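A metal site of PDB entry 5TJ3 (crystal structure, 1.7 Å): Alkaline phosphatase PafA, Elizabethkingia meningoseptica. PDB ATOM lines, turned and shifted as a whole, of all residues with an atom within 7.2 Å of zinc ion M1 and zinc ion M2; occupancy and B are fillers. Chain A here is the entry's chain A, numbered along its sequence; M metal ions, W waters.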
ATOM      1  N   VAL A  25      24.791   5.220  -9.393  1.00  0.00           N
ATOM      2  CA  VAL A  25      24.710   5.983 -10.625  1.00  0.00           C
ATOM      3  C   VAL A  25      25.369   5.159 -11.727  1.00  0.00           C
ATOM      4  O   VAL A  25      26.563   4.841 -11.661  1.00  0.00           O
ATOM      5  CB  VAL A  25      25.325   7.386 -10.488  1.00  0.00           C
ATOM      6  CG1 VAL A  25      26.085   7.545  -9.186  1.00  0.00           C
ATOM      7  CG2 VAL A  25      26.129   7.801 -11.717  1.00  0.00           C
ATOM      8  N   VAL A  26      24.557   4.758 -12.709  1.00  0.00           N
ATOM      9  CA  VAL A  26      25.004   3.928 -13.818  1.00  0.00           C
ATOM     10  C   VAL A  26      25.578   4.865 -14.873  1.00  0.00           C
ATOM     11  O   VAL A  26      24.860   5.676 -15.466  1.00  0.00           O
ATOM     12  CB  VAL A  26      23.857   3.097 -14.400  1.00  0.00           C
ATOM     13  CG1 VAL A  26      24.363   2.223 -15.539  1.00  0.00           C
ATOM     14  CG2 VAL A  26      23.229   2.253 -13.301  1.00  0.00           C
ATOM     15  N   ASP A  27      26.881   4.764 -15.097  1.00  0.00           N
ATOM     16  CA  ASP A  27      27.583   5.731 -15.920  1.00  0.00           C
ATOM     17  C   ASP A  27      27.125   5.628 -17.370  1.00  0.00           C
ATOM     18  O   ASP A  27      27.135   4.548 -17.966  1.00  0.00           O
ATOM     19  CB  ASP A  27      29.086   5.499 -15.799  1.00  0.00           C
ATOM     20  CG  ASP A  27      29.881   6.742 -16.067  1.00  0.00           C
ATOM     21  OD1 ASP A  27      29.537   7.443 -17.037  1.00  0.00           O
ATOM     22  OD2 ASP A  27      30.832   7.017 -15.309  1.00  0.00           O
ATOM     23  N   GLN A  28      26.693   6.763 -17.930  1.00  0.00           N
ATOM     24  CA  GLN A  28      26.253   6.906 -19.316  1.00  0.00           C
ATOM     25  C   GLN A  28      24.919   6.216 -19.593  1.00  0.00           C
ATOM     26  O   GLN A  28      24.614   5.899 -20.745  1.00  0.00           O
ATOM     27  CB  GLN A  28      27.315   6.392 -20.308  1.00  0.00           C
ATOM     28  CG  GLN A  28      27.273   7.080 -21.663  1.00  0.00           C
ATOM     29  CD  GLN A  28      28.166   6.396 -22.691  1.00  0.00           C
ATOM     30  OE1 GLN A  28      27.666   5.694 -23.574  1.00  0.00           O
ATOM     31  NE2 GLN A  28      29.472   6.599 -22.577  1.00  0.00           N
ATOM     32  N   MET A  29      24.104   5.971 -18.570  1.00  0.00           N
ATOM     33  CA  MET A  29      22.832   5.280 -18.795  1.00  0.00           C
ATOM     34  C   MET A  29      21.791   6.272 -19.283  1.00  0.00           C
ATOM     35  O   MET A  29      21.265   7.070 -18.512  1.00  0.00           O
ATOM     36  CB  MET A  29      22.365   4.584 -17.522  1.00  0.00           C
ATOM     37  CG  MET A  29      21.078   3.832 -17.745  1.00  0.00           C
ATOM     38  SD  MET A  29      20.582   2.857 -16.318  1.00  0.00           S
ATOM     39  CE  MET A  29      19.109   2.080 -16.977  1.00  0.00           C
ATOM     40  N   THR A  66      27.624  17.813 -19.913  1.00  0.00           N
ATOM     41  CA  THR A  66      27.110  16.602 -19.275  1.00  0.00           C
ATOM     42  C   THR A  66      28.192  15.513 -19.269  1.00  0.00           C
ATOM     43  O   THR A  66      28.140  14.530 -19.992  1.00  0.00           O
ATOM     44  CB  THR A  66      25.833  16.135 -19.952  1.00  0.00           C
ATOM     45  OG1 THR A  66      26.039  16.082 -21.378  1.00  0.00           O
ATOM     46  CG2 THR A  66      24.690  17.089 -19.651  1.00  0.00           C
ATOM     47  N   VAL A  67      29.193  15.736 -18.407  1.00  0.00           N
ATOM     48  CA  VAL A  67      30.277  14.784 -18.233  1.00  0.00           C
ATOM     49  C   VAL A  67      30.252  14.177 -16.827  1.00  0.00           C
ATOM     50  O   VAL A  67      29.427  14.559 -16.003  1.00  0.00           O
ATOM     51  CB  VAL A  67      31.636  15.440 -18.521  1.00  0.00           C
ATOM     52  CG1 VAL A  67      31.647  16.017 -19.925  1.00  0.00           C
ATOM     53  CG2 VAL A  67      31.941  16.506 -17.493  1.00  0.00           C
ATOM     54  N   TPO A  68      31.166  13.245 -16.569  1.00  0.00           N
ATOM     55  CA  TPO A  68      31.146  12.417 -15.359  1.00  0.00           C
ATOM     56  CB  TPO A  68      32.152  11.292 -15.475  1.00  0.00           C
ATOM     57  CG2 TPO A  68      32.365  10.595 -14.133  1.00  0.00           C
ATOM     58  OG1 TPO A  68      31.647  10.348 -16.394  1.00  0.00           O
ATOM     59  P   TPO A  68      32.664  10.343 -17.646  1.00  0.00           P
ATOM     60  O1P TPO A  68      32.819  11.707 -18.215  1.00  0.00           O
ATOM     61  O2P TPO A  68      34.091   9.809 -17.137  1.00  0.00           O
ATOM     62  O3P TPO A  68      32.049   9.350 -18.740  1.00  0.00           O
ATOM     63  C   TPO A  68      31.360  13.167 -14.053  1.00  0.00           C
ATOM     64  O   TPO A  68      30.540  13.068 -13.132  1.00  0.00           O
ATOM     65  N   ALA A  69      32.474  13.881 -13.963  1.00  0.00           N
ATOM     66  CA  ALA A  69      32.854  14.552 -12.721  1.00  0.00           C
ATOM     67  C   ALA A  69      31.733  15.460 -12.247  1.00  0.00           C
ATOM     68  O   ALA A  69      31.404  15.473 -11.060  1.00  0.00           O
ATOM     69  CB  ALA A  69      34.138  15.331 -12.894  1.00  0.00           C
ATOM     70  N   GLY A  71      28.496  15.293 -13.195  1.00  0.00           N
ATOM     71  CA  GLY A  71      27.296  14.512 -12.931  1.00  0.00           C
ATOM     72  C   GLY A  71      27.277  13.924 -11.533  1.00  0.00           C
ATOM     73  O   GLY A  71      26.298  14.074 -10.802  1.00  0.00           O
ATOM     74  N   HIS A  72      28.366  13.266 -11.147  1.00  0.00           N
ATOM     75  CA  HIS A  72      28.431  12.705  -9.797  1.00  0.00           C
ATOM     76  C   HIS A  72      28.438  13.807  -8.749  1.00  0.00           C
ATOM     77  O   HIS A  72      27.804  13.671  -7.694  1.00  0.00           O
ATOM     78  CB  HIS A  72      29.650  11.805  -9.670  1.00  0.00           C
ATOM     79  CG  HIS A  72      29.520  10.503 -10.398  1.00  0.00           C
ATOM     80  ND1 HIS A  72      29.710  10.383 -11.755  1.00  0.00           N
ATOM     81  CD2 HIS A  72      29.152   9.279  -9.959  1.00  0.00           C
ATOM     82  CE1 HIS A  72      29.498   9.136 -12.118  1.00  0.00           C
ATOM     83  NE2 HIS A  72      29.163   8.440 -11.046  1.00  0.00           N
ATOM     84  N   ASN A  89      35.450  17.030 -16.066  1.00  0.00           N
ATOM     85  CA  ASN A  89      36.494  16.067 -15.740  1.00  0.00           C
ATOM     86  C   ASN A  89      37.858  16.750 -15.693  1.00  0.00           C
ATOM     87  O   ASN A  89      38.705  16.422 -14.871  1.00  0.00           O
ATOM     88  CB  ASN A  89      36.516  14.927 -16.749  1.00  0.00           C
ATOM     89  CG  ASN A  89      35.244  14.101 -16.724  1.00  0.00           C
ATOM     90  OD1 ASN A  89      34.567  14.017 -15.709  1.00  0.00           O
ATOM     91  ND2 ASN A  89      34.910  13.477 -17.852  1.00  0.00           N
ATOM     92  N   LYS A 151      36.443   4.363 -11.409  1.00  0.00           N
ATOM     93  CA  LYS A 151      37.013   5.674 -11.684  1.00  0.00           C
ATOM     94  C   LYS A 151      37.226   6.437 -10.382  1.00  0.00           C
ATOM     95  O   LYS A 151      36.338   6.477  -9.526  1.00  0.00           O
ATOM     96  CB  LYS A 151      36.112   6.504 -12.599  1.00  0.00           C
ATOM     97  CG  LYS A 151      35.685   5.851 -13.892  1.00  0.00           C
ATOM     98  CD  LYS A 151      34.709   6.769 -14.617  1.00  0.00           C
ATOM     99  CE  LYS A 151      34.328   6.230 -15.979  1.00  0.00           C
ATOM    100  NZ  LYS A 151      33.468   7.180 -16.740  1.00  0.00           N
ATOM    101  N   ARG A 153      37.308   9.720  -9.968  1.00  0.00           N
ATOM    102  CA  ARG A 153      36.380  10.853  -9.860  1.00  0.00           C
ATOM    103  C   ARG A 153      34.999  10.396  -9.419  1.00  0.00           C
ATOM    104  O   ARG A 153      34.317  11.099  -8.659  1.00  0.00           O
ATOM    105  CB  ARG A 153      36.309  11.601 -11.186  1.00  0.00           C
ATOM    106  CG  ARG A 153      35.995  10.738 -12.410  1.00  0.00           C
ATOM    107  CD  ARG A 153      36.087  11.561 -13.688  1.00  0.00           C
ATOM    108  NE  ARG A 153      35.806  10.794 -14.898  1.00  0.00           N
ATOM    109  CZ  ARG A 153      36.734  10.141 -15.589  1.00  0.00           C
ATOM    110  NH1 ARG A 153      37.995  10.150 -15.195  1.00  0.00           N
ATOM    111  NH2 ARG A 153      36.392   9.466 -16.688  1.00  0.00           N
ATOM    112  N   ALA A 154      34.559   9.232  -9.879  1.00  0.00           N
ATOM    113  CA  ALA A 154      33.210   8.750  -9.587  1.00  0.00           C
ATOM    114  C   ALA A 154      33.099   8.091  -8.210  1.00  0.00           C
ATOM    115  O   ALA A 154      31.976   7.776  -7.786  1.00  0.00           O
ATOM    116  CB  ALA A 154      32.758   7.770 -10.667  1.00  0.00           C
ATOM    117  N   ASN A 289      29.393   3.887  -8.264  1.00  0.00           N
ATOM    118  CA  ASN A 289      29.246   4.207  -9.677  1.00  0.00           C
ATOM    119  C   ASN A 289      29.554   2.968 -10.488  1.00  0.00           C
ATOM    120  O   ASN A 289      30.575   2.307 -10.259  1.00  0.00           O
ATOM    121  CB  ASN A 289      30.181   5.353 -10.060  1.00  0.00           C
ATOM    122  CG  ASN A 289      30.596   5.300 -11.522  1.00  0.00           C
ATOM    123  OD1 ASN A 289      31.596   4.672 -11.870  1.00  0.00           O
ATOM    124  ND2 ASN A 289      29.836   5.966 -12.369  1.00  0.00           N
ATOM    125  N   ALA A 291      30.793   2.013 -13.772  1.00  0.00           N
ATOM    126  CA  ALA A 291      31.496   2.738 -14.815  1.00  0.00           C
ATOM    127  C   ALA A 291      31.551   2.006 -16.152  1.00  0.00           C
ATOM    128  O   ALA A 291      31.748   2.660 -17.191  1.00  0.00           O
ATOM    129  CB  ALA A 291      32.917   3.069 -14.371  1.00  0.00           C
ATOM    130  N   ASP A 294      29.758   3.042 -19.261  1.00  0.00           N
ATOM    131  CA  ASP A 294      30.326   4.203 -19.948  1.00  0.00           C
ATOM    132  C   ASP A 294      31.481   3.812 -20.851  1.00  0.00           C
ATOM    133  O   ASP A 294      31.576   4.273 -21.986  1.00  0.00           O
ATOM    134  CB  ASP A 294      30.790   5.233 -18.920  1.00  0.00           C
ATOM    135  CG  ASP A 294      31.378   6.466 -19.550  1.00  0.00           C
ATOM    136  OD1 ASP A 294      30.603   7.281 -20.100  1.00  0.00           O
ATOM    137  OD2 ASP A 294      32.621   6.624 -19.494  1.00  0.00           O
ATOM    138  N   TYR A 295      32.382   2.966 -20.350  1.00  0.00           N
ATOM    139  CA  TYR A 295      33.504   2.504 -21.168  1.00  0.00           C
ATOM    140  C   TYR A 295      32.994   1.715 -22.365  1.00  0.00           C
ATOM    141  O   TYR A 295      33.423   1.946 -23.505  1.00  0.00           O
ATOM    142  CB  TYR A 295      34.462   1.667 -20.327  1.00  0.00           C
ATOM    143  CG  TYR A 295      35.294   2.495 -19.386  1.00  0.00           C
ATOM    144  CD1 TYR A 295      36.381   3.222 -19.844  1.00  0.00           C
ATOM    145  CD2 TYR A 295      35.003   2.551 -18.027  1.00  0.00           C
ATOM    146  CE1 TYR A 295      37.151   3.989 -18.987  1.00  0.00           C
ATOM    147  CE2 TYR A 295      35.762   3.308 -17.154  1.00  0.00           C
ATOM    148  CZ  TYR A 295      36.840   4.022 -17.649  1.00  0.00           C
ATOM    149  OH  TYR A 295      37.608   4.786 -16.801  1.00  0.00           O
ATOM    150  N   HIS A 298      31.217   4.134 -24.749  1.00  0.00           N
ATOM    151  CA  HIS A 298      32.164   4.979 -25.465  1.00  0.00           C
ATOM    152  C   HIS A 298      32.777   4.257 -26.656  1.00  0.00           C
ATOM    153  O   HIS A 298      33.052   4.863 -27.696  1.00  0.00           O
ATOM    154  CB  HIS A 298      33.265   5.448 -24.524  1.00  0.00           C
ATOM    155  CG  HIS A 298      32.969   6.745 -23.832  1.00  0.00           C
ATOM    156  ND1 HIS A 298      32.896   7.942 -24.512  1.00  0.00           N
ATOM    157  CD2 HIS A 298      32.741   7.024 -22.531  1.00  0.00           C
ATOM    158  CE1 HIS A 298      32.623   8.903 -23.647  1.00  0.00           C
ATOM    159  NE2 HIS A 298      32.527   8.374 -22.445  1.00  0.00           N
ATOM    160  N   ALA A 340      21.833   8.350 -13.358  1.00  0.00           N
ATOM    161  CA  ALA A 340      22.986   8.356 -14.233  1.00  0.00           C
ATOM    162  C   ALA A 340      23.599   9.744 -14.209  1.00  0.00           C
ATOM    163  O   ALA A 340      22.927  10.732 -13.903  1.00  0.00           O
ATOM    164  CB  ALA A 340      22.606   7.972 -15.669  1.00  0.00           C
ATOM    165  N   ASP A 341      24.888   9.811 -14.509  1.00  0.00           N
ATOM    166  CA  ASP A 341      25.552  11.113 -14.575  1.00  0.00           C
ATOM    167  C   ASP A 341      25.335  11.807 -15.905  1.00  0.00           C
ATOM    168  O   ASP A 341      25.622  13.010 -16.006  1.00  0.00           O
ATOM    169  CB  ASP A 341      27.047  10.949 -14.292  1.00  0.00           C
ATOM    170  CG  ASP A 341      27.706   9.900 -15.168  1.00  0.00           C
ATOM    171  OD1 ASP A 341      27.000   9.081 -15.784  1.00  0.00           O
ATOM    172  OD2 ASP A 341      28.953   9.890 -15.218  1.00  0.00           O
ATOM    173  N   HIS A 342      24.817  11.087 -16.907  1.00  0.00           N
ATOM    174  CA  HIS A 342      24.503  11.606 -18.232  1.00  0.00           C
ATOM    175  C   HIS A 342      24.031  10.464 -19.124  1.00  0.00           C
ATOM    176  O   HIS A 342      24.133   9.295 -18.751  1.00  0.00           O
ATOM    177  CB  HIS A 342      25.731  12.260 -18.869  1.00  0.00           C
ATOM    178  CG  HIS A 342      26.946  11.389 -18.836  1.00  0.00           C
ATOM    179  ND1 HIS A 342      27.092  10.297 -19.673  1.00  0.00           N
ATOM    180  CD2 HIS A 342      28.045  11.400 -18.042  1.00  0.00           C
ATOM    181  CE1 HIS A 342      28.237   9.699 -19.405  1.00  0.00           C
ATOM    182  NE2 HIS A 342      28.831  10.351 -18.417  1.00  0.00           N
ATOM    183  N   GLY A 343      23.494  10.791 -20.293  1.00  0.00           N
ATOM    184  CA  GLY A 343      23.177   9.815 -21.317  1.00  0.00           C
ATOM    185  C   GLY A 343      24.300   9.687 -22.323  1.00  0.00           C
ATOM    186  O   GLY A 343      25.487   9.788 -21.977  1.00  0.00           O
ATOM    187  N   THR A 473      30.903   6.501 -29.176  1.00  0.00           N
ATOM    188  CA  THR A 473      30.097   7.703 -28.945  1.00  0.00           C
ATOM    189  C   THR A 473      30.695   8.482 -27.775  1.00  0.00           C
ATOM    190  O   THR A 473      31.688   8.082 -27.175  1.00  0.00           O
ATOM    191  CB  THR A 473      28.625   7.348 -28.702  1.00  0.00           C
ATOM    192  OG1 THR A 473      27.833   8.529 -28.812  1.00  0.00           O
ATOM    193  CG2 THR A 473      28.452   6.743 -27.308  1.00  0.00           C
ATOM    194  N   THR A 474      30.061   9.612 -27.471  1.00  0.00           N
ATOM    195  CA  THR A 474      30.488  10.465 -26.364  1.00  0.00           C
ATOM    196  C   THR A 474      29.284  11.271 -25.893  1.00  0.00           C
ATOM    197  O   THR A 474      28.157  11.074 -26.359  1.00  0.00           O
ATOM    198  CB  THR A 474      31.665  11.353 -26.778  1.00  0.00           C
ATOM    199  OG1 THR A 474      32.199  12.016 -25.630  1.00  0.00           O
ATOM    200  CG2 THR A 474      31.215  12.390 -27.796  1.00  0.00           C
ATOM    201  N   HIS A 475      29.534  12.207 -24.981  1.00  0.00           N
ATOM    202  CA  HIS A 475      28.468  12.893 -24.261  1.00  0.00           C
ATOM    203  C   HIS A 475      29.026  14.182 -23.664  1.00  0.00           C
ATOM    204  O   HIS A 475      30.120  14.164 -23.096  1.00  0.00           O
ATOM    205  CB  HIS A 475      27.944  11.987 -23.142  1.00  0.00           C
ATOM    206  CG  HIS A 475      29.018  11.563 -22.196  1.00  0.00           C
ATOM    207  ND1 HIS A 475      29.482  12.373 -21.180  1.00  0.00           N
ATOM    208  CD2 HIS A 475      29.768  10.434 -22.148  1.00  0.00           C
ATOM    209  CE1 HIS A 475      30.442  11.753 -20.520  1.00  0.00           C
ATOM    210  NE2 HIS A 475      30.636  10.578 -21.091  1.00  0.00           N
HETATM  211 ZN    ZN M   1      31.969   8.963 -20.574  1.00  0.00          ZN
HETATM  212 ZN    ZN M   2      29.948   9.360 -16.912  1.00  0.00          ZN
HETATM  213  O   HOH W   1      34.082  10.162 -20.411  1.00  0.00           O
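O2P of TPO 68 lies within salt-bridge range of the side-chain amino group (NZ) of Lys 151. The guanidinium group of Arg 153 lies within salt-bridge range of O2P of TPO 68 (3.0 Å). The side-chain amide nitrogen (ND2) of Asn 89 is in hydrogen-bond range of O1P of TPO 68 (2.8 Å). OD1 of Asp 341 sits at hydrogen-bond distance from N of Gln 28 (3.2 Å). A ring nitrogen (NE2) of His 342 lies close to a ring nitrogen (ND1) of His 475 (3.5 Å). O of His 342 sits at hydrogen-bond distance from N of Met 29. ND1 of His 475 lies within hydrogen-bond range of O of Thr 66, 2.8 Å away. OD2 of Asp 294 is in salt-bridge range of NZ of Lys 151, at 2.9 Å.
Zinc ion M1 is bound by O3P of TPO 68 (1.9 Å), a ring nitrogen (NE2) of His 298 (2.0 Å), a ring nitrogen (NE2) of His 475 (2.2 Å), the side-chain carboxylate of Asp 294 (2.2 Å) and water W1 (2.4 Å). Zinc ion M1 has five donor atoms within binding distance. Slightly farther from zinc ion M1 lies the side-chain carboxylate (OD2) of Asp 294 (2.7 Å).
Zinc ion M2 is bound by the side-chain carboxylate (OD1) of Asp 27 (2.0 Å), OG1 of TPO 68 (2.0 Å), the side-chain carboxylate (OD2) of Asp 341 (2.0 Å) and a ring nitrogen (NE2) of His 342 (2.1 Å). Slightly farther from zinc ion M2 lies O3P of TPO 68 (2.8 Å).
Gln 28 touches zinc ion M1 (NE2 to ZN, 3.98 Å). Of the 27 residues printed, 6 come within 4 Å of zinc ion M1.
Of the 27 residues printed, 5 come within 4 Å of zinc ion M2. The nearest printed residue that does not touch zinc ion M2 is Lys 151 (4.1 Å).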
